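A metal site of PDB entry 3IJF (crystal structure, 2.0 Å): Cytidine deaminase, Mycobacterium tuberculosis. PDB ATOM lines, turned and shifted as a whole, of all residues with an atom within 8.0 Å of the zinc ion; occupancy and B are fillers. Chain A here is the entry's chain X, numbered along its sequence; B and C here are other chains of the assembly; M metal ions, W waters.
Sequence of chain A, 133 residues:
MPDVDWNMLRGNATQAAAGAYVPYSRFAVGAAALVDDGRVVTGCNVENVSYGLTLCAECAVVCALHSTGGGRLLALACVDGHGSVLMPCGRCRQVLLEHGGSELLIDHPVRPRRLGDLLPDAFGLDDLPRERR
SG of Cys 89 sits close to N of Arg 91, at 3.6 Å.
OE2 of Glu 58 sits close to SG of Cys 78, at 3.6 Å.
The guanidinium group of Arg 91 lies close to the side-chain sulfur of Cys 56 (3.4 Å).
SG of Cys 56 sits close to OG of Ser 50 of chain B.
SG of Cys 92 lies close to OE2 of Glu 58 (3.6 Å).
SG of Cys 89 sits close to OG of Ser 50 of chain B (3.3 Å).
OE2 of Glu 58 touches the zinc ion, at 3.7 Å.
Four residues have an atom within 4 Å of the zinc ion: Cys 56, Glu 58, Cys 89 and Cys 92.
The zinc ion is bound by water W1, SG of Cys 89, SG of Cys 92 and SG of Cys 56.
The zinc ion has four donor atoms within binding distance.
Water W1 bridges OE2 of Glu 58 (2.7 Å) and N of Cys 89 (2.9 Å).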
ATOM      1  N   VAL A  29      30.139 -31.066 -14.907  1.00  0.00           N
ATOM      2  CA  VAL A  29      30.896 -30.213 -13.971  1.00  0.00           C
ATOM      3  C   VAL A  29      31.586 -31.116 -12.980  1.00  0.00           C
ATOM      4  O   VAL A  29      30.975 -32.031 -12.479  1.00  0.00           O
ATOM      5  CB  VAL A  29      29.993 -29.226 -13.179  1.00  0.00           C
ATOM      6  CG1 VAL A  29      30.855 -28.331 -12.282  1.00  0.00           C
ATOM      7  CG2 VAL A  29      29.129 -28.374 -14.134  1.00  0.00           C
ATOM      8  N   ASN A  45      28.563 -33.070 -10.931  1.00  0.00           N
ATOM      9  CA  ASN A  45      27.192 -32.856 -11.380  1.00  0.00           C
ATOM     10  C   ASN A  45      26.276 -34.126 -11.420  1.00  0.00           C
ATOM     11  O   ASN A  45      26.642 -35.105 -12.023  1.00  0.00           O
ATOM     12  CB  ASN A  45      27.349 -32.321 -12.853  1.00  0.00           C
ATOM     13  CG  ASN A  45      26.583 -31.136 -13.033  1.00  0.00           C
ATOM     14  OD1 ASN A  45      26.054 -30.655 -12.020  1.00  0.00           O
ATOM     15  ND2 ASN A  45      26.448 -30.631 -14.258  1.00  0.00           N
ATOM     16  N   THR A  54      18.584 -31.600  -9.462  1.00  0.00           N
ATOM     17  CA  THR A  54      20.009 -31.781  -9.801  1.00  0.00           C
ATOM     18  C   THR A  54      20.973 -31.293  -8.740  1.00  0.00           C
ATOM     19  O   THR A  54      20.794 -30.219  -8.107  1.00  0.00           O
ATOM     20  CB  THR A  54      20.457 -31.418 -11.287  1.00  0.00           C
ATOM     21  OG1 THR A  54      21.667 -30.600 -11.400  1.00  0.00           O
ATOM     22  CG2 THR A  54      19.362 -31.068 -12.169  1.00  0.00           C
ATOM     23  N   LEU A  55      21.964 -32.143  -8.534  1.00  0.00           N
ATOM     24  CA  LEU A  55      23.013 -31.923  -7.580  1.00  0.00           C
ATOM     25  C   LEU A  55      24.220 -31.282  -8.267  1.00  0.00           C
ATOM     26  O   LEU A  55      24.631 -31.721  -9.311  1.00  0.00           O
ATOM     27  CB  LEU A  55      23.366 -33.286  -6.960  1.00  0.00           C
ATOM     28  CG  LEU A  55      22.174 -33.842  -6.171  1.00  0.00           C
ATOM     29  CD1 LEU A  55      22.099 -35.377  -6.182  1.00  0.00           C
ATOM     30  CD2 LEU A  55      22.277 -33.263  -4.729  1.00  0.00           C
ATOM     31  N   CYS A  56      24.720 -30.207  -7.694  1.00  0.00           N
ATOM     32  CA  CYS A  56      25.927 -29.591  -8.177  1.00  0.00           C
ATOM     33  C   CYS A  56      27.142 -30.333  -7.687  1.00  0.00           C
ATOM     34  O   CYS A  56      27.155 -30.914  -6.572  1.00  0.00           O
ATOM     35  CB  CYS A  56      26.027 -28.171  -7.657  1.00  0.00           C
ATOM     36  SG  CYS A  56      25.038 -27.067  -8.668  1.00  0.00           S
ATOM     37  N   ALA A  57      28.155 -30.319  -8.536  1.00  0.00           N
ATOM     38  CA  ALA A  57      29.436 -30.934  -8.239  1.00  0.00           C
ATOM     39  C   ALA A  57      30.011 -30.385  -6.926  1.00  0.00           C
ATOM     40  O   ALA A  57      30.553 -31.155  -6.131  1.00  0.00           O
ATOM     41  CB  ALA A  57      30.416 -30.735  -9.423  1.00  0.00           C
ATOM     42  N   GLU A  58      29.890 -29.087  -6.688  1.00  0.00           N
ATOM     43  CA  GLU A  58      30.474 -28.462  -5.464  1.00  0.00           C
ATOM     44  C   GLU A  58      29.728 -28.870  -4.202  1.00  0.00           C
ATOM     45  O   GLU A  58      30.326 -29.009  -3.092  1.00  0.00           O
ATOM     46  CB  GLU A  58      30.570 -26.915  -5.605  1.00  0.00           C
ATOM     47  CG  GLU A  58      31.168 -26.472  -6.981  1.00  0.00           C
ATOM     48  CD  GLU A  58      30.084 -26.208  -8.053  1.00  0.00           C
ATOM     49  OE1 GLU A  58      29.443 -27.151  -8.528  1.00  0.00           O
ATOM     50  OE2 GLU A  58      29.871 -25.046  -8.440  1.00  0.00           O
ATOM     51  N   CYS A  59      28.437 -29.153  -4.388  1.00  0.00           N
ATOM     52  CA  CYS A  59      27.612 -29.730  -3.332  1.00  0.00           C
ATOM     53  C   CYS A  59      28.012 -31.158  -3.116  1.00  0.00           C
ATOM     54  O   CYS A  59      28.080 -31.589  -1.994  1.00  0.00           O
ATOM     55  CB  CYS A  59      26.135 -29.682  -3.698  1.00  0.00           C
ATOM     56  SG  CYS A  59      25.466 -28.071  -3.638  1.00  0.00           S
ATOM     57  N   CYS A  78      36.601 -25.774  -9.541  1.00  0.00           N
ATOM     58  CA  CYS A  78      35.422 -26.272 -10.250  1.00  0.00           C
ATOM     59  C   CYS A  78      35.672 -26.162 -11.760  1.00  0.00           C
ATOM     60  O   CYS A  78      36.172 -25.168 -12.216  1.00  0.00           O
ATOM     61  CB  CYS A  78      34.180 -25.474  -9.829  1.00  0.00           C
ATOM     62  SG  CYS A  78      32.625 -26.021 -10.605  1.00  0.00           S
ATOM     63  N   MET A  87      33.074 -20.790 -12.414  1.00  0.00           N
ATOM     64  CA  MET A  87      32.737 -20.239 -11.106  1.00  0.00           C
ATOM     65  C   MET A  87      31.527 -21.008 -10.646  1.00  0.00           C
ATOM     66  O   MET A  87      30.644 -21.301 -11.462  1.00  0.00           O
ATOM     67  CB  MET A  87      32.440 -18.728 -11.144  1.00  0.00           C
ATOM     68  CG  MET A  87      33.651 -17.794 -11.421  1.00  0.00           C
ATOM     69  SD  MET A  87      34.944 -17.999 -10.232  1.00  0.00           S
ATOM     70  CE  MET A  87      36.041 -19.074 -11.153  1.00  0.00           C
ATOM     71  N   PRO A  88      31.476 -21.333  -9.372  1.00  0.00           N
ATOM     72  CA  PRO A  88      30.346 -22.031  -8.805  1.00  0.00           C
ATOM     73  C   PRO A  88      29.083 -21.201  -8.944  1.00  0.00           C
ATOM     74  O   PRO A  88      29.131 -19.960  -8.851  1.00  0.00           O
ATOM     75  CB  PRO A  88      30.748 -22.166  -7.314  1.00  0.00           C
ATOM     76  CG  PRO A  88      32.284 -22.239  -7.386  1.00  0.00           C
ATOM     77  CD  PRO A  88      32.530 -21.112  -8.357  1.00  0.00           C
ATOM     78  N   CYS A  89      27.965 -21.871  -9.166  1.00  0.00           N
ATOM     79  CA  CYS A  89      26.697 -21.180  -9.139  1.00  0.00           C
ATOM     80  C   CYS A  89      26.443 -20.586  -7.729  1.00  0.00           C
ATOM     81  O   CYS A  89      27.146 -20.909  -6.754  1.00  0.00           O
ATOM     82  CB  CYS A  89      25.554 -22.103  -9.606  1.00  0.00           C
ATOM     83  SG  CYS A  89      24.935 -23.204  -8.317  1.00  0.00           S
ATOM     84  N   GLY A  90      25.481 -19.676  -7.638  1.00  0.00           N
ATOM     85  CA  GLY A  90      25.214 -18.965  -6.374  1.00  0.00           C
ATOM     86  C   GLY A  90      24.913 -19.921  -5.234  1.00  0.00           C
ATOM     87  O   GLY A  90      25.364 -19.720  -4.091  1.00  0.00           O
ATOM     88  N   ARG A  91      24.172 -20.990  -5.550  1.00  0.00           N
ATOM     89  CA  ARG A  91      23.786 -22.016  -4.559  1.00  0.00           C
ATOM     90  C   ARG A  91      25.010 -22.683  -3.997  1.00  0.00           C
ATOM     91  O   ARG A  91      25.105 -22.898  -2.767  1.00  0.00           O
ATOM     92  CB  ARG A  91      22.820 -23.076  -5.130  1.00  0.00           C
ATOM     93  CG  ARG A  91      22.923 -24.462  -4.422  1.00  0.00           C
ATOM     94  CD  ARG A  91      22.975 -25.727  -5.394  1.00  0.00           C
ATOM     95  NE  ARG A  91      21.705 -26.521  -5.268  1.00  0.00           N
ATOM     96  CZ  ARG A  91      21.259 -27.367  -6.186  1.00  0.00           C
ATOM     97  NH1 ARG A  91      21.981 -27.506  -7.277  1.00  0.00           N
ATOM     98  NH2 ARG A  91      20.099 -28.079  -6.013  1.00  0.00           N
ATOM     99  N   CYS A  92      25.966 -22.960  -4.886  1.00  0.00           N
ATOM    100  CA  CYS A  92      27.195 -23.603  -4.478  1.00  0.00           C
ATOM    101  C   CYS A  92      28.035 -22.660  -3.699  1.00  0.00           C
ATOM    102  O   CYS A  92      28.633 -23.063  -2.700  1.00  0.00           O
ATOM    103  CB  CYS A  92      27.947 -24.148  -5.692  1.00  0.00           C
ATOM    104  SG  CYS A  92      27.103 -25.634  -6.158  1.00  0.00           S
ATOM    105  N   ARG A  93      28.052 -21.386  -4.075  1.00  0.00           N
ATOM    106  CA  ARG A  93      28.803 -20.409  -3.294  1.00  0.00           C
ATOM    107  C   ARG A  93      28.306 -20.335  -1.820  1.00  0.00           C
ATOM    108  O   ARG A  93      29.093 -20.305  -0.900  1.00  0.00           O
ATOM    109  CB  ARG A  93      28.714 -19.041  -3.929  1.00  0.00           C
ATOM    110  CG  ARG A  93      29.436 -18.964  -5.246  1.00  0.00           C
ATOM    111  CD  ARG A  93      29.430 -17.586  -5.867  1.00  0.00           C
ATOM    112  NE  ARG A  93      29.770 -17.671  -7.299  1.00  0.00           N
ATOM    113  CZ  ARG A  93      30.051 -16.623  -8.067  1.00  0.00           C
ATOM    114  NH1 ARG A  93      30.052 -15.382  -7.574  1.00  0.00           N
ATOM    115  NH2 ARG A  93      30.352 -16.810  -9.349  1.00  0.00           N
ATOM    116  N   VAL A  95      26.647 -22.872  -0.289  1.00  0.00           N
ATOM    117  CA  VAL A  95      26.933 -24.082   0.471  1.00  0.00           C
ATOM    118  C   VAL A  95      28.425 -24.183   0.803  1.00  0.00           C
ATOM    119  O   VAL A  95      28.776 -24.532   1.932  1.00  0.00           O
ATOM    120  CB  VAL A  95      26.275 -25.476  -0.055  1.00  0.00           C
ATOM    121  CG1 VAL A  95      25.055 -25.243  -0.900  1.00  0.00           C
ATOM    122  CG2 VAL A  95      27.286 -26.434  -0.642  1.00  0.00           C
ATOM    123  N   LEU A  96      29.305 -23.823  -0.144  1.00  0.00           N
ATOM    124  CA  LEU A  96      30.765 -23.812   0.133  1.00  0.00           C
ATOM    125  C   LEU A  96      31.137 -22.926   1.335  1.00  0.00           C
ATOM    126  O   LEU A  96      31.938 -23.310   2.192  1.00  0.00           O
ATOM    127  CB  LEU A  96      31.531 -23.392  -1.109  1.00  0.00           C
ATOM    128  CG  LEU A  96      31.417 -24.466  -2.194  1.00  0.00           C
ATOM    129  CD1 LEU A  96      31.938 -23.918  -3.526  1.00  0.00           C
ATOM    130  CD2 LEU A  96      32.096 -25.795  -1.760  1.00  0.00           C
ATOM    131  N   SER B  50      21.592 -23.072 -13.652  1.00  0.00           N
ATOM    132  CA  SER B  50      21.996 -24.069 -12.718  1.00  0.00           C
ATOM    133  C   SER B  50      20.727 -24.834 -12.525  1.00  0.00           C
ATOM    134  O   SER B  50      19.795 -24.371 -11.837  1.00  0.00           O
ATOM    135  CB  SER B  50      22.501 -23.464 -11.406  1.00  0.00           C
ATOM    136  OG  SER B  50      23.025 -24.528 -10.599  1.00  0.00           O
ATOM    137  N   TYR B  51      20.654 -26.001 -13.173  1.00  0.00           N
ATOM    138  CA  TYR B  51      19.405 -26.809 -13.175  1.00  0.00           C
ATOM    139  C   TYR B  51      18.812 -27.038 -11.813  1.00  0.00           C
ATOM    140  O   TYR B  51      17.591 -27.008 -11.667  1.00  0.00           O
ATOM    141  CB  TYR B  51      19.595 -28.150 -13.838  1.00  0.00           C
ATOM    142  CG  TYR B  51      19.553 -28.101 -15.358  1.00  0.00           C
ATOM    143  CD1 TYR B  51      19.755 -26.894 -16.048  1.00  0.00           C
ATOM    144  CD2 TYR B  51      19.406 -29.266 -16.101  1.00  0.00           C
ATOM    145  CE1 TYR B  51      19.771 -26.833 -17.456  1.00  0.00           C
ATOM    146  CE2 TYR B  51      19.419 -29.231 -17.546  1.00  0.00           C
ATOM    147  CZ  TYR B  51      19.586 -27.980 -18.193  1.00  0.00           C
ATOM    148  OH  TYR B  51      19.597 -27.887 -19.574  1.00  0.00           O
ATOM    149  N   GLY B  52      19.644 -27.309 -10.815  1.00  0.00           N
ATOM    150  CA  GLY B  52      19.140 -27.678  -9.503  1.00  0.00           C
ATOM    151  C   GLY B  52      18.506 -26.513  -8.786  1.00  0.00           C
ATOM    152  O   GLY B  52      18.043 -26.658  -7.668  1.00  0.00           O
ATOM    153  N   LEU B  53      18.502 -25.330  -9.425  1.00  0.00           N
ATOM    154  CA  LEU B  53      17.845 -24.192  -8.787  1.00  0.00           C
ATOM    155  C   LEU B  53      16.461 -23.990  -9.386  1.00  0.00           C
ATOM    156  O   LEU B  53      15.751 -23.107  -8.974  1.00  0.00           O
ATOM    157  CB  LEU B  53      18.705 -22.926  -8.910  1.00  0.00           C
ATOM    158  CG  LEU B  53      20.154 -23.086  -8.433  1.00  0.00           C
ATOM    159  CD1 LEU B  53      20.758 -21.696  -8.253  1.00  0.00           C
ATOM    160  CD2 LEU B  53      20.297 -23.917  -7.191  1.00  0.00           C
ATOM    161  N   GLN C  94      21.790 -16.451  -7.609  1.00  0.00           N
ATOM    162  CA  GLN C  94      21.694 -17.165  -8.875  1.00  0.00           C
ATOM    163  C   GLN C  94      20.289 -17.153  -9.484  1.00  0.00           C
ATOM    164  O   GLN C  94      20.156 -16.932 -10.686  1.00  0.00           O
ATOM    165  CB  GLN C  94      22.197 -18.602  -8.701  1.00  0.00           C
ATOM    166  CG  GLN C  94      22.629 -19.284 -10.060  1.00  0.00           C
ATOM    167  CD  GLN C  94      23.920 -18.765 -10.587  1.00  0.00           C
ATOM    168  OE1 GLN C  94      24.910 -18.681  -9.872  1.00  0.00           O
ATOM    169  NE2 GLN C  94      23.919 -18.424 -11.856  1.00  0.00           N
ATOM    170  N   PHE C 123      28.144 -17.846 -12.669  1.00  0.00           N
ATOM    171  CA  PHE C 123      27.835 -18.956 -13.579  1.00  0.00           C
ATOM    172  C   PHE C 123      26.506 -18.584 -14.245  1.00  0.00           C
ATOM    173  O   PHE C 123      25.674 -17.899 -13.646  1.00  0.00           O
ATOM    174  CB  PHE C 123      27.752 -20.264 -12.770  1.00  0.00           C
ATOM    175  CG  PHE C 123      27.223 -21.445 -13.544  1.00  0.00           C
ATOM    176  CD1 PHE C 123      28.084 -22.288 -14.234  1.00  0.00           C
ATOM    177  CD2 PHE C 123      25.852 -21.716 -13.564  1.00  0.00           C
ATOM    178  CE1 PHE C 123      27.573 -23.391 -14.965  1.00  0.00           C
ATOM    179  CE2 PHE C 123      25.352 -22.802 -14.287  1.00  0.00           C
ATOM    180  CZ  PHE C 123      26.200 -23.648 -14.987  1.00  0.00           C
HETATM  181 ZN    ZN M   1      26.139 -25.103  -8.151  1.00  0.00          ZN
HETATM  182  O   HOH W   1      27.578 -24.644  -9.731  1.00  0.00           O
